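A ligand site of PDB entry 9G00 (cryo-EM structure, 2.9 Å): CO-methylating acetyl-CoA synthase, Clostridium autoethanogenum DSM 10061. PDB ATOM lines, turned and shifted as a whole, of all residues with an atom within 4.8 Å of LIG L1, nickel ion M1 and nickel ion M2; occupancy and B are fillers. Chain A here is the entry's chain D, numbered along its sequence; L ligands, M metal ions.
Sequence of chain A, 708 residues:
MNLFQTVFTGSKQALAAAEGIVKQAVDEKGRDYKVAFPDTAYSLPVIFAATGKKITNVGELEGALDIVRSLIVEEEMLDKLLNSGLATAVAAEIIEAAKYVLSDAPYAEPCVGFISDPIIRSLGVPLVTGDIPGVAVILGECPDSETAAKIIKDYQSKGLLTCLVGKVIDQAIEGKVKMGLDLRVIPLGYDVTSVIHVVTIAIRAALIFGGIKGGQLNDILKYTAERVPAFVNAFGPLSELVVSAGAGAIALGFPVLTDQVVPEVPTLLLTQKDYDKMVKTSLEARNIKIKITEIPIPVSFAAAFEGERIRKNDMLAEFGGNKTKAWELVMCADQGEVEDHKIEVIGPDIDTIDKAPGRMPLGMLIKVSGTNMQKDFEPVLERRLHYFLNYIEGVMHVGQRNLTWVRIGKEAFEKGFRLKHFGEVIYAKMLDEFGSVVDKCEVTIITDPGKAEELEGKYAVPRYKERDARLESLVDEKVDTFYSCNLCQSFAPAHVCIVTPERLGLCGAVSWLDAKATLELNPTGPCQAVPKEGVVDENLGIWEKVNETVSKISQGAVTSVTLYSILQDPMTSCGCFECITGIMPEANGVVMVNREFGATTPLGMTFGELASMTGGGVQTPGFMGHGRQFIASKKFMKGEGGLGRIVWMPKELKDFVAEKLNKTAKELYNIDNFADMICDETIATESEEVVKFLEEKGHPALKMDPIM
Within 4 Å of nickel ion M1: Cys 488, Cys 574 and Cys 576.
Along chain A the residues within 4 Å of nickel ion M1 span positions 488 to 576.
The nearest printed residue that does not touch nickel ion M1 is His 495 (4.2 Å).
A sulfur (S2) of LIG L1 lies close to a nitrogen (N5) of LG2 L2 (3.5 Å).
His 495 touches LIG L1 (NE2 to FE2, 3.99 Å).
Leu 506 touches LIG L1 (N to S1, 3.9 Å).
Val 510 touches LIG L1.
Hydrophobic or aromatic side chains that line LIG L1: Leu 487 and Val 510.
Ten residues have an atom within 4 Å of LIG L1: Cys 485, Leu 487, Cys 488, His 495, Cys 497, Leu 506, Cys 507, Val 510, Cys 574 and Cys 576.
The nearest printed residue that does not touch LIG L1 is Asn 486 (4.1 Å).
Nickel ion M2 is bound by the backbone nitrogen (N) of Cys 576, the backbone nitrogen (N) of Gly 575, the side-chain sulfur (SG) of Cys 574 and the side-chain sulfur (SG) of Cys 576.
Phe 577 touches nickel ion M2.
Four residues have an atom within 4 Å of nickel ion M2: Cys 574, Gly 575, Cys 576 and Phe 577.
The nearest printed residue that does not touch nickel ion M2 is Phe 491 (4.3 Å).
SG of Cys 576 is bound to nickel ion M1 (2.0 Å).
Nickel ion M1 is bound by SG of Cys 574, at 2.1 Å.
The side-chain sulfur (SG) of Cys 488 binds nickel ion M1 (2.1 Å).
Nickel ion M1 is bound by a sulfur (S1) of LIG L1 (2.4 Å).
Nickel ion M1 has four donor atoms within binding distance.
A sulfur (S3) of LIG L1 sits close to the backbone NH (N) of Cys 488 (3.4 Å).
An iron atom (FE4) of LIG L1 is bound by the side-chain sulfur of Cys 488.
SG of Cys 507 sits close to N5 of LG2 L2 (3.2 Å).
SG of Cys 485 is bound to FE1 of LIG L1 (2.3 Å).
SG of Cys 497 is bound to FE2 of LIG L1 (2.4 Å).
N of Cys 507 sits close to S1 of LIG L1, at 3.6 Å.
N7 of LG2 L2 sits at hydrogen-bond distance from O of Cys 576 (2.7 Å).
An iron atom (FE3) of LIG L1 is bound by the side-chain sulfur (SG) of Cys 507.
The backbone NH (N) of Leu 487 lies close to a sulfur (S3) of LIG L1, 3.5 Å away.
The backbone NH (N) of Gly 505 lies within hydrogen-bond range of the backbone carbonyl oxygen (O) of Val 510 (2.8 Å).
The side-chain sulfur of Cys 497 lies close to a ring nitrogen (NE2) of His 495 (2.9 Å).
The backbone carbonyl oxygen (O) of Cys 497 sits at hydrogen-bond distance from the backbone NH (N) of Cys 485, at 2.9 Å.
SG of Cys 485 sits close to N of Leu 487 (3.8 Å).
A ring nitrogen (NE2) of His 495 sits close to the side-chain sulfur (SG) of Cys 574 (3.4 Å).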
ATOM      1  N   CYS A 485     -23.918  10.693 -19.490  1.00  0.00           N
ATOM      2  CA  CYS A 485     -25.067  10.145 -18.793  1.00  0.00           C
ATOM      3  C   CYS A 485     -25.901  11.286 -18.233  1.00  0.00           C
ATOM      4  O   CYS A 485     -25.362  12.294 -17.751  1.00  0.00           O
ATOM      5  CB  CYS A 485     -24.617   9.221 -17.669  1.00  0.00           C
ATOM      6  SG  CYS A 485     -25.956   8.438 -16.743  1.00  0.00           S
ATOM      7  N   ASN A 486     -27.228  11.159 -18.322  1.00  0.00           N
ATOM      8  CA  ASN A 486     -28.140  12.200 -17.846  1.00  0.00           C
ATOM      9  C   ASN A 486     -29.304  11.593 -17.095  1.00  0.00           C
ATOM     10  O   ASN A 486     -30.451  12.038 -17.228  1.00  0.00           O
ATOM     11  CB  ASN A 486     -28.647  13.042 -19.013  1.00  0.00           C
ATOM     12  CG  ASN A 486     -29.438  12.241 -19.998  1.00  0.00           C
ATOM     13  OD1 ASN A 486     -29.364  11.015 -20.026  1.00  0.00           O
ATOM     14  ND2 ASN A 486     -30.217  12.921 -20.826  1.00  0.00           N
ATOM     15  N   LEU A 487     -29.035  10.569 -16.288  1.00  0.00           N
ATOM     16  CA  LEU A 487     -30.089   9.955 -15.502  1.00  0.00           C
ATOM     17  C   LEU A 487     -30.370  10.687 -14.191  1.00  0.00           C
ATOM     18  O   LEU A 487     -31.365  10.369 -13.528  1.00  0.00           O
ATOM     19  CB  LEU A 487     -29.752   8.498 -15.196  1.00  0.00           C
ATOM     20  CG  LEU A 487     -30.697   7.445 -15.765  1.00  0.00           C
ATOM     21  CD1 LEU A 487     -30.271   6.060 -15.345  1.00  0.00           C
ATOM     22  CD2 LEU A 487     -32.127   7.696 -15.330  1.00  0.00           C
ATOM     23  N   CYS A 488     -29.519  11.620 -13.795  1.00  0.00           N
ATOM     24  CA  CYS A 488     -29.746  12.421 -12.599  1.00  0.00           C
ATOM     25  C   CYS A 488     -30.373  13.765 -12.903  1.00  0.00           C
ATOM     26  O   CYS A 488     -30.496  14.601 -11.998  1.00  0.00           O
ATOM     27  CB  CYS A 488     -28.435  12.629 -11.829  1.00  0.00           C
ATOM     28  SG  CYS A 488     -27.837  11.164 -10.950  1.00  0.00           S
ATOM     29  N   PHE A 491     -33.685  15.573 -11.038  1.00  0.00           N
ATOM     30  CA  PHE A 491     -33.646  16.581  -9.986  1.00  0.00           C
ATOM     31  C   PHE A 491     -32.545  17.613 -10.149  1.00  0.00           C
ATOM     32  O   PHE A 491     -32.546  18.610  -9.429  1.00  0.00           O
ATOM     33  CB  PHE A 491     -33.483  15.917  -8.611  1.00  0.00           C
ATOM     34  CG  PHE A 491     -32.161  15.231  -8.420  1.00  0.00           C
ATOM     35  CD1 PHE A 491     -31.956  13.958  -8.931  1.00  0.00           C
ATOM     36  CD2 PHE A 491     -31.141  15.835  -7.725  1.00  0.00           C
ATOM     37  CE1 PHE A 491     -30.752  13.328  -8.750  1.00  0.00           C
ATOM     38  CE2 PHE A 491     -29.941  15.192  -7.545  1.00  0.00           C
ATOM     39  CZ  PHE A 491     -29.753  13.941  -8.062  1.00  0.00           C
ATOM     40  N   HIS A 495     -27.369  19.036 -15.141  1.00  0.00           N
ATOM     41  CA  HIS A 495     -26.251  18.153 -14.866  1.00  0.00           C
ATOM     42  C   HIS A 495     -26.058  17.132 -15.986  1.00  0.00           C
ATOM     43  O   HIS A 495     -26.997  16.408 -16.344  1.00  0.00           O
ATOM     44  CB  HIS A 495     -26.475  17.412 -13.553  1.00  0.00           C
ATOM     45  CG  HIS A 495     -25.411  16.396 -13.256  1.00  0.00           C
ATOM     46  ND1 HIS A 495     -24.081  16.727 -13.155  1.00  0.00           N
ATOM     47  CD2 HIS A 495     -25.492  15.059 -13.058  1.00  0.00           C
ATOM     48  CE1 HIS A 495     -23.383  15.639 -12.895  1.00  0.00           C
ATOM     49  NE2 HIS A 495     -24.211  14.617 -12.829  1.00  0.00           N
ATOM     50  N   CYS A 497     -23.091  14.139 -16.854  1.00  0.00           N
ATOM     51  CA  CYS A 497     -21.908  13.404 -16.424  1.00  0.00           C
ATOM     52  C   CYS A 497     -21.138  12.944 -17.661  1.00  0.00           C
ATOM     53  O   CYS A 497     -21.688  12.221 -18.493  1.00  0.00           O
ATOM     54  CB  CYS A 497     -22.280  12.192 -15.573  1.00  0.00           C
ATOM     55  SG  CYS A 497     -22.515  12.529 -13.821  1.00  0.00           S
ATOM     56  N   VAL A 499     -18.276  10.582 -18.817  1.00  0.00           N
ATOM     57  CA  VAL A 499     -17.665   9.361 -18.302  1.00  0.00           C
ATOM     58  C   VAL A 499     -16.481   9.022 -19.189  1.00  0.00           C
ATOM     59  O   VAL A 499     -16.632   8.839 -20.405  1.00  0.00           O
ATOM     60  CB  VAL A 499     -18.667   8.203 -18.233  1.00  0.00           C
ATOM     61  CG1 VAL A 499     -17.984   6.928 -17.807  1.00  0.00           C
ATOM     62  CG2 VAL A 499     -19.796   8.540 -17.280  1.00  0.00           C
ATOM     63  N   GLY A 505     -18.595   7.826 -13.228  1.00  0.00           N
ATOM     64  CA  GLY A 505     -19.672   8.700 -12.816  1.00  0.00           C
ATOM     65  C   GLY A 505     -19.548   9.131 -11.365  1.00  0.00           C
ATOM     66  O   GLY A 505     -18.848   8.530 -10.561  1.00  0.00           O
ATOM     67  N   LEU A 506     -20.258  10.213 -11.035  1.00  0.00           N
ATOM     68  CA  LEU A 506     -20.224  10.724  -9.671  1.00  0.00           C
ATOM     69  C   LEU A 506     -20.807   9.727  -8.695  1.00  0.00           C
ATOM     70  O   LEU A 506     -20.279   9.551  -7.585  1.00  0.00           O
ATOM     71  CB  LEU A 506     -20.967  12.054  -9.580  1.00  0.00           C
ATOM     72  CG  LEU A 506     -20.624  13.106 -10.629  1.00  0.00           C
ATOM     73  CD1 LEU A 506     -21.277  14.414 -10.254  1.00  0.00           C
ATOM     74  CD2 LEU A 506     -19.122  13.282 -10.773  1.00  0.00           C
ATOM     75  N   CYS A 507     -21.891   9.054  -9.071  1.00  0.00           N
ATOM     76  CA  CYS A 507     -22.484   8.058  -8.189  1.00  0.00           C
ATOM     77  C   CYS A 507     -21.583   6.848  -8.021  1.00  0.00           C
ATOM     78  O   CYS A 507     -21.752   6.112  -7.042  1.00  0.00           O
ATOM     79  CB  CYS A 507     -23.831   7.624  -8.749  1.00  0.00           C
ATOM     80  SG  CYS A 507     -23.778   7.106 -10.473  1.00  0.00           S
ATOM     81  N   VAL A 510     -21.545   3.935 -12.557  1.00  0.00           N
ATOM     82  CA  VAL A 510     -21.443   3.977 -14.007  1.00  0.00           C
ATOM     83  C   VAL A 510     -19.985   4.238 -14.370  1.00  0.00           C
ATOM     84  O   VAL A 510     -19.392   5.192 -13.868  1.00  0.00           O
ATOM     85  CB  VAL A 510     -22.360   5.044 -14.619  1.00  0.00           C
ATOM     86  CG1 VAL A 510     -22.173   5.124 -16.123  1.00  0.00           C
ATOM     87  CG2 VAL A 510     -23.801   4.748 -14.296  1.00  0.00           C
ATOM     88  N   CYS A 574     -24.615  16.441  -9.231  1.00  0.00           N
ATOM     89  CA  CYS A 574     -26.046  16.246  -8.990  1.00  0.00           C
ATOM     90  C   CYS A 574     -26.354  16.162  -7.505  1.00  0.00           C
ATOM     91  O   CYS A 574     -27.000  17.061  -6.949  1.00  0.00           O
ATOM     92  CB  CYS A 574     -26.528  14.977  -9.703  1.00  0.00           C
ATOM     93  SG  CYS A 574     -25.304  13.660  -9.785  1.00  0.00           S
ATOM     94  N   GLY A 575     -25.808  15.171  -6.814  1.00  0.00           N
ATOM     95  CA  GLY A 575     -26.173  14.963  -5.423  1.00  0.00           C
ATOM     96  C   GLY A 575     -26.030  13.536  -4.961  1.00  0.00           C
ATOM     97  O   GLY A 575     -26.212  13.229  -3.779  1.00  0.00           O
ATOM     98  N   CYS A 576     -25.711  12.654  -5.899  1.00  0.00           N
ATOM     99  CA  CYS A 576     -25.419  11.261  -5.599  1.00  0.00           C
ATOM    100  C   CYS A 576     -23.985  11.021  -5.185  1.00  0.00           C
ATOM    101  O   CYS A 576     -23.665   9.913  -4.725  1.00  0.00           O
ATOM    102  CB  CYS A 576     -25.734  10.428  -6.834  1.00  0.00           C
ATOM    103  SG  CYS A 576     -25.276  11.248  -8.371  1.00  0.00           S
ATOM    104  N   PHE A 577     -23.125  12.025  -5.300  1.00  0.00           N
ATOM    105  CA  PHE A 577     -21.715  11.853  -4.964  1.00  0.00           C
ATOM    106  C   PHE A 577     -21.533  11.482  -3.501  1.00  0.00           C
ATOM    107  O   PHE A 577     -22.225  11.999  -2.624  1.00  0.00           O
ATOM    108  CB  PHE A 577     -20.945  13.134  -5.289  1.00  0.00           C
ATOM    109  CG  PHE A 577     -21.641  14.387  -4.845  1.00  0.00           C
ATOM    110  CD1 PHE A 577     -21.578  14.813  -3.534  1.00  0.00           C
ATOM    111  CD2 PHE A 577     -22.372  15.136  -5.742  1.00  0.00           C
ATOM    112  CE1 PHE A 577     -22.230  15.959  -3.135  1.00  0.00           C
ATOM    113  CE2 PHE A 577     -23.015  16.279  -5.346  1.00  0.00           C
ATOM    114  CZ  PHE A 577     -22.947  16.696  -4.045  1.00  0.00           C
HETATM  115 FE1  LIG L   1     -25.893   8.920 -14.544  1.00  0.00          FE
HETATM  116 FE2  LIG L   1     -24.022  10.722 -13.683  1.00  0.00          FE
HETATM  117 FE3  LIG L   1     -24.369   8.366 -12.341  1.00  0.00          FE
HETATM  118 FE4  LIG L   1     -26.299  10.308 -12.231  1.00  0.00          FE
HETATM  119  S1  LIG L   1     -24.169  10.453 -11.426  1.00  0.00           S
HETATM  120  S2  LIG L   1     -26.623   8.077 -12.564  1.00  0.00           S
HETATM  121  S3  LIG L   1     -26.163  11.175 -14.332  1.00  0.00           S
HETATM  122  S4  LIG L   1     -23.636   8.622 -14.482  1.00  0.00           S
HETATM  123 CO1  LG2 L   2     -29.627   7.575  -6.624  1.00  0.00          CO
HETATM  124  N1  LG2 L   2     -29.315   5.960  -7.520  1.00  0.00           N
HETATM  125  N2  LG2 L   2     -28.149   7.227  -5.437  1.00  0.00           N
HETATM  126  N3  LG2 L   2     -30.149   9.217  -5.940  1.00  0.00           N
HETATM  127  N4  LG2 L   2     -31.021   7.689  -7.926  1.00  0.00           N
HETATM  128  C1  LG2 L   2     -30.257   5.498  -8.570  1.00  0.00           C
HETATM  129  C2  LG2 L   2     -31.417   4.681  -7.901  1.00  0.00           C
HETATM  130  C3  LG2 L   2     -29.355   4.577  -9.469  1.00  0.00           C
HETATM  131  C4  LG2 L   2     -30.158   3.610 -10.406  1.00  0.00           C
HETATM  132  C5  LG2 L   2     -28.378   5.453 -10.279  1.00  0.00           C
HETATM  133  C6  LG2 L   2     -27.410   4.617 -11.115  1.00  0.00           C
HETATM  134  O1  LG2 L   2     -27.717   3.684 -11.856  1.00  0.00           O
HETATM  135  N5  LG2 L   2     -26.133   4.990 -10.985  1.00  0.00           N
HETATM  136  C7  LG2 L   2     -28.546   3.861  -8.351  1.00  0.00           C
HETATM  137  C8  LG2 L   2     -29.024   2.534  -7.684  1.00  0.00           C
HETATM  138  C9  LG2 L   2     -27.979   1.373  -7.771  1.00  0.00           C
HETATM  139  C10 LG2 L   2     -28.159   0.264  -6.740  1.00  0.00           C
HETATM  140  O2  LG2 L   2     -28.504   0.527  -5.580  1.00  0.00           O
HETATM  141  N6  LG2 L   2     -27.942  -0.998  -7.126  1.00  0.00           N
HETATM  142  C11 LG2 L   2     -28.442   4.987  -7.304  1.00  0.00           C
HETATM  143  C12 LG2 L   2     -27.406   5.048  -6.289  1.00  0.00           C
HETATM  144  C13 LG2 L   2     -26.498   3.852  -6.277  1.00  0.00           C
HETATM  145  C14 LG2 L   2     -27.282   6.107  -5.401  1.00  0.00           C
HETATM  146  C15 LG2 L   2     -26.247   6.285  -4.291  1.00  0.00           C
HETATM  147  C16 LG2 L   2     -26.224   5.111  -3.283  1.00  0.00           C
HETATM  148  C17 LG2 L   2     -24.820   6.490  -4.945  1.00  0.00           C
HETATM  149  C18 LG2 L   2     -23.691   6.585  -3.861  1.00  0.00           C
HETATM  150  O3  LG2 L   2     -22.992   5.608  -3.686  1.00  0.00           O
HETATM  151  N7  LG2 L   2     -23.488   7.700  -3.163  1.00  0.00           N
HETATM  152  C19 LG2 L   2     -26.638   7.617  -3.636  1.00  0.00           C
HETATM  153  C20 LG2 L   2     -27.079   7.508  -2.118  1.00  0.00           C
HETATM  154  C21 LG2 L   2     -27.133   8.852  -1.377  1.00  0.00           C
HETATM  155  C22 LG2 L   2     -27.127   8.681   0.103  1.00  0.00           C
HETATM  156  O4  LG2 L   2     -26.578   7.684   0.614  1.00  0.00           O
HETATM  157  N8  LG2 L   2     -27.722   9.575   0.912  1.00  0.00           N
HETATM  158  C23 LG2 L   2     -27.806   8.073  -4.497  1.00  0.00           C
HETATM  159  C24 LG2 L   2     -28.458   9.244  -4.258  1.00  0.00           C
HETATM  160  C25 LG2 L   2     -29.514   9.787  -4.890  1.00  0.00           C
HETATM  161  C26 LG2 L   2     -30.060  11.161  -4.534  1.00  0.00           C
HETATM  162  C27 LG2 L   2     -28.936  12.181  -4.914  1.00  0.00           C
HETATM  163  C28 LG2 L   2     -30.381  11.248  -3.016  1.00  0.00           C
HETATM  164  C29 LG2 L   2     -31.265  11.261  -5.438  1.00  0.00           C
HETATM  165  C30 LG2 L   2     -32.668  11.202  -4.713  1.00  0.00           C
HETATM  166  C31 LG2 L   2     -33.257  12.611  -4.555  1.00  0.00           C
HETATM  167  C32 LG2 L   2     -34.780  12.449  -4.522  1.00  0.00           C
HETATM  168  O5  LG2 L   2     -35.329  11.537  -3.801  1.00  0.00           O
HETATM  169  N9  LG2 L   2     -35.429  13.256  -5.275  1.00  0.00           N
HETATM  170  C33 LG2 L   2     -31.162  10.042  -6.335  1.00  0.00           C
HETATM  171  C34 LG2 L   2     -32.033   9.788  -7.377  1.00  0.00           C
HETATM  172  C35 LG2 L   2     -33.137  10.777  -7.727  1.00  0.00           C
HETATM  173  C36 LG2 L   2     -31.964   8.566  -8.109  1.00  0.00           C
HETATM  174  C37 LG2 L   2     -32.764   8.213  -9.389  1.00  0.00           C
HETATM  175  C38 LG2 L   2     -32.224   9.267 -10.395  1.00  0.00           C
HETATM  176  C39 LG2 L   2     -34.271   8.304  -9.361  1.00  0.00           C
HETATM  177  C40 LG2 L   2     -35.013   7.635  -8.196  1.00  0.00           C
HETATM  178  C41 LG2 L   2     -36.524   7.661  -8.468  1.00  0.00           C
HETATM  179  O6  LG2 L   2     -37.198   8.621  -8.125  1.00  0.00           O
HETATM  180  N10 LG2 L   2     -37.019   6.639  -9.135  1.00  0.00           N
HETATM  181  C42 LG2 L   2     -32.265   6.811  -9.721  1.00  0.00           C
HETATM  182  C43 LG2 L   2     -32.285   6.371 -11.218  1.00  0.00           C
HETATM  183  C44 LG2 L   2     -33.066   5.081 -11.471  1.00  0.00           C
HETATM  184  O7  LG2 L   2     -33.920   4.661 -10.679  1.00  0.00           O
HETATM  185  N11 LG2 L   2     -32.744   4.476 -12.608  1.00  0.00           N
HETATM  186  C45 LG2 L   2     -30.870   6.805  -9.122  1.00  0.00           C
HETATM  187  C46 LG2 L   2     -38.443   6.553  -9.518  1.00  0.00           C
HETATM  188  C47 LG2 L   2     -39.369   6.269  -8.333  1.00  0.00           C
HETATM  189  C48 LG2 L   2     -40.814   6.683  -8.647  1.00  0.00           C
HETATM  190  O8  LG2 L   2     -39.384   4.824  -8.179  1.00  0.00           O
HETATM  191  O9  LG2 L   2     -39.312   5.209  -5.687  1.00  0.00           O
HETATM  192  O10 LG2 L   2     -38.887   2.854  -6.710  1.00  0.00           O
HETATM  193  P1  LG2 L   2     -39.612   4.190  -6.705  1.00  0.00           P
HETATM  194  O11 LG2 L   2     -41.215   3.838  -6.659  1.00  0.00           O
HETATM  195  C49 LG2 L   2     -41.825   2.967  -7.566  1.00  0.00           C
HETATM  196  C50 LG2 L   2     -41.830   1.503  -7.135  1.00  0.00           C
HETATM  197  O12 LG2 L   2     -41.123   1.214  -5.969  1.00  0.00           O
HETATM  198  C51 LG2 L   2     -43.339   1.117  -7.010  1.00  0.00           C
HETATM  199  O13 LG2 L   2     -44.047   2.139  -7.650  1.00  0.00           O
HETATM  200  C52 LG2 L   2     -43.330   3.378  -7.529  1.00  0.00           C
HETATM  201  C53 LG2 L   2     -43.752   4.336  -8.640  1.00  0.00           C
HETATM  202  O14 LG2 L   2     -43.664   3.626  -9.916  1.00  0.00           O
HETATM  203  N12 LG2 L   2     -43.875   0.963  -5.651  1.00  0.00           N
HETATM  204  C54 LG2 L   2     -44.859   0.051  -5.345  1.00  0.00           C
HETATM  205  C55 LG2 L   2     -43.603   1.598  -4.519  1.00  0.00           C
HETATM  206  N13 LG2 L   2     -44.320   1.156  -3.500  1.00  0.00           N
HETATM  207  C56 LG2 L   2     -45.158   0.148  -4.002  1.00  0.00           C
HETATM  208  C57 LG2 L   2     -46.135  -0.697  -3.456  1.00  0.00           C
HETATM  209  C58 LG2 L   2     -46.798  -1.621  -4.260  1.00  0.00           C
HETATM  210  C59 LG2 L   2     -47.861  -2.532  -3.693  1.00  0.00           C
HETATM  211  C60 LG2 L   2     -46.502  -1.730  -5.633  1.00  0.00           C
HETATM  212  C61 LG2 L   2     -47.152  -2.675  -6.572  1.00  0.00           C
HETATM  213  C62 LG2 L   2     -45.516  -0.874  -6.166  1.00  0.00           C
HETATM  214 NI    NI M   1     -25.858  11.660 -10.289  1.00  0.00          NI
HETATM  215 NI    NI M   2     -25.552  13.338  -7.635  1.00  0.00          NI
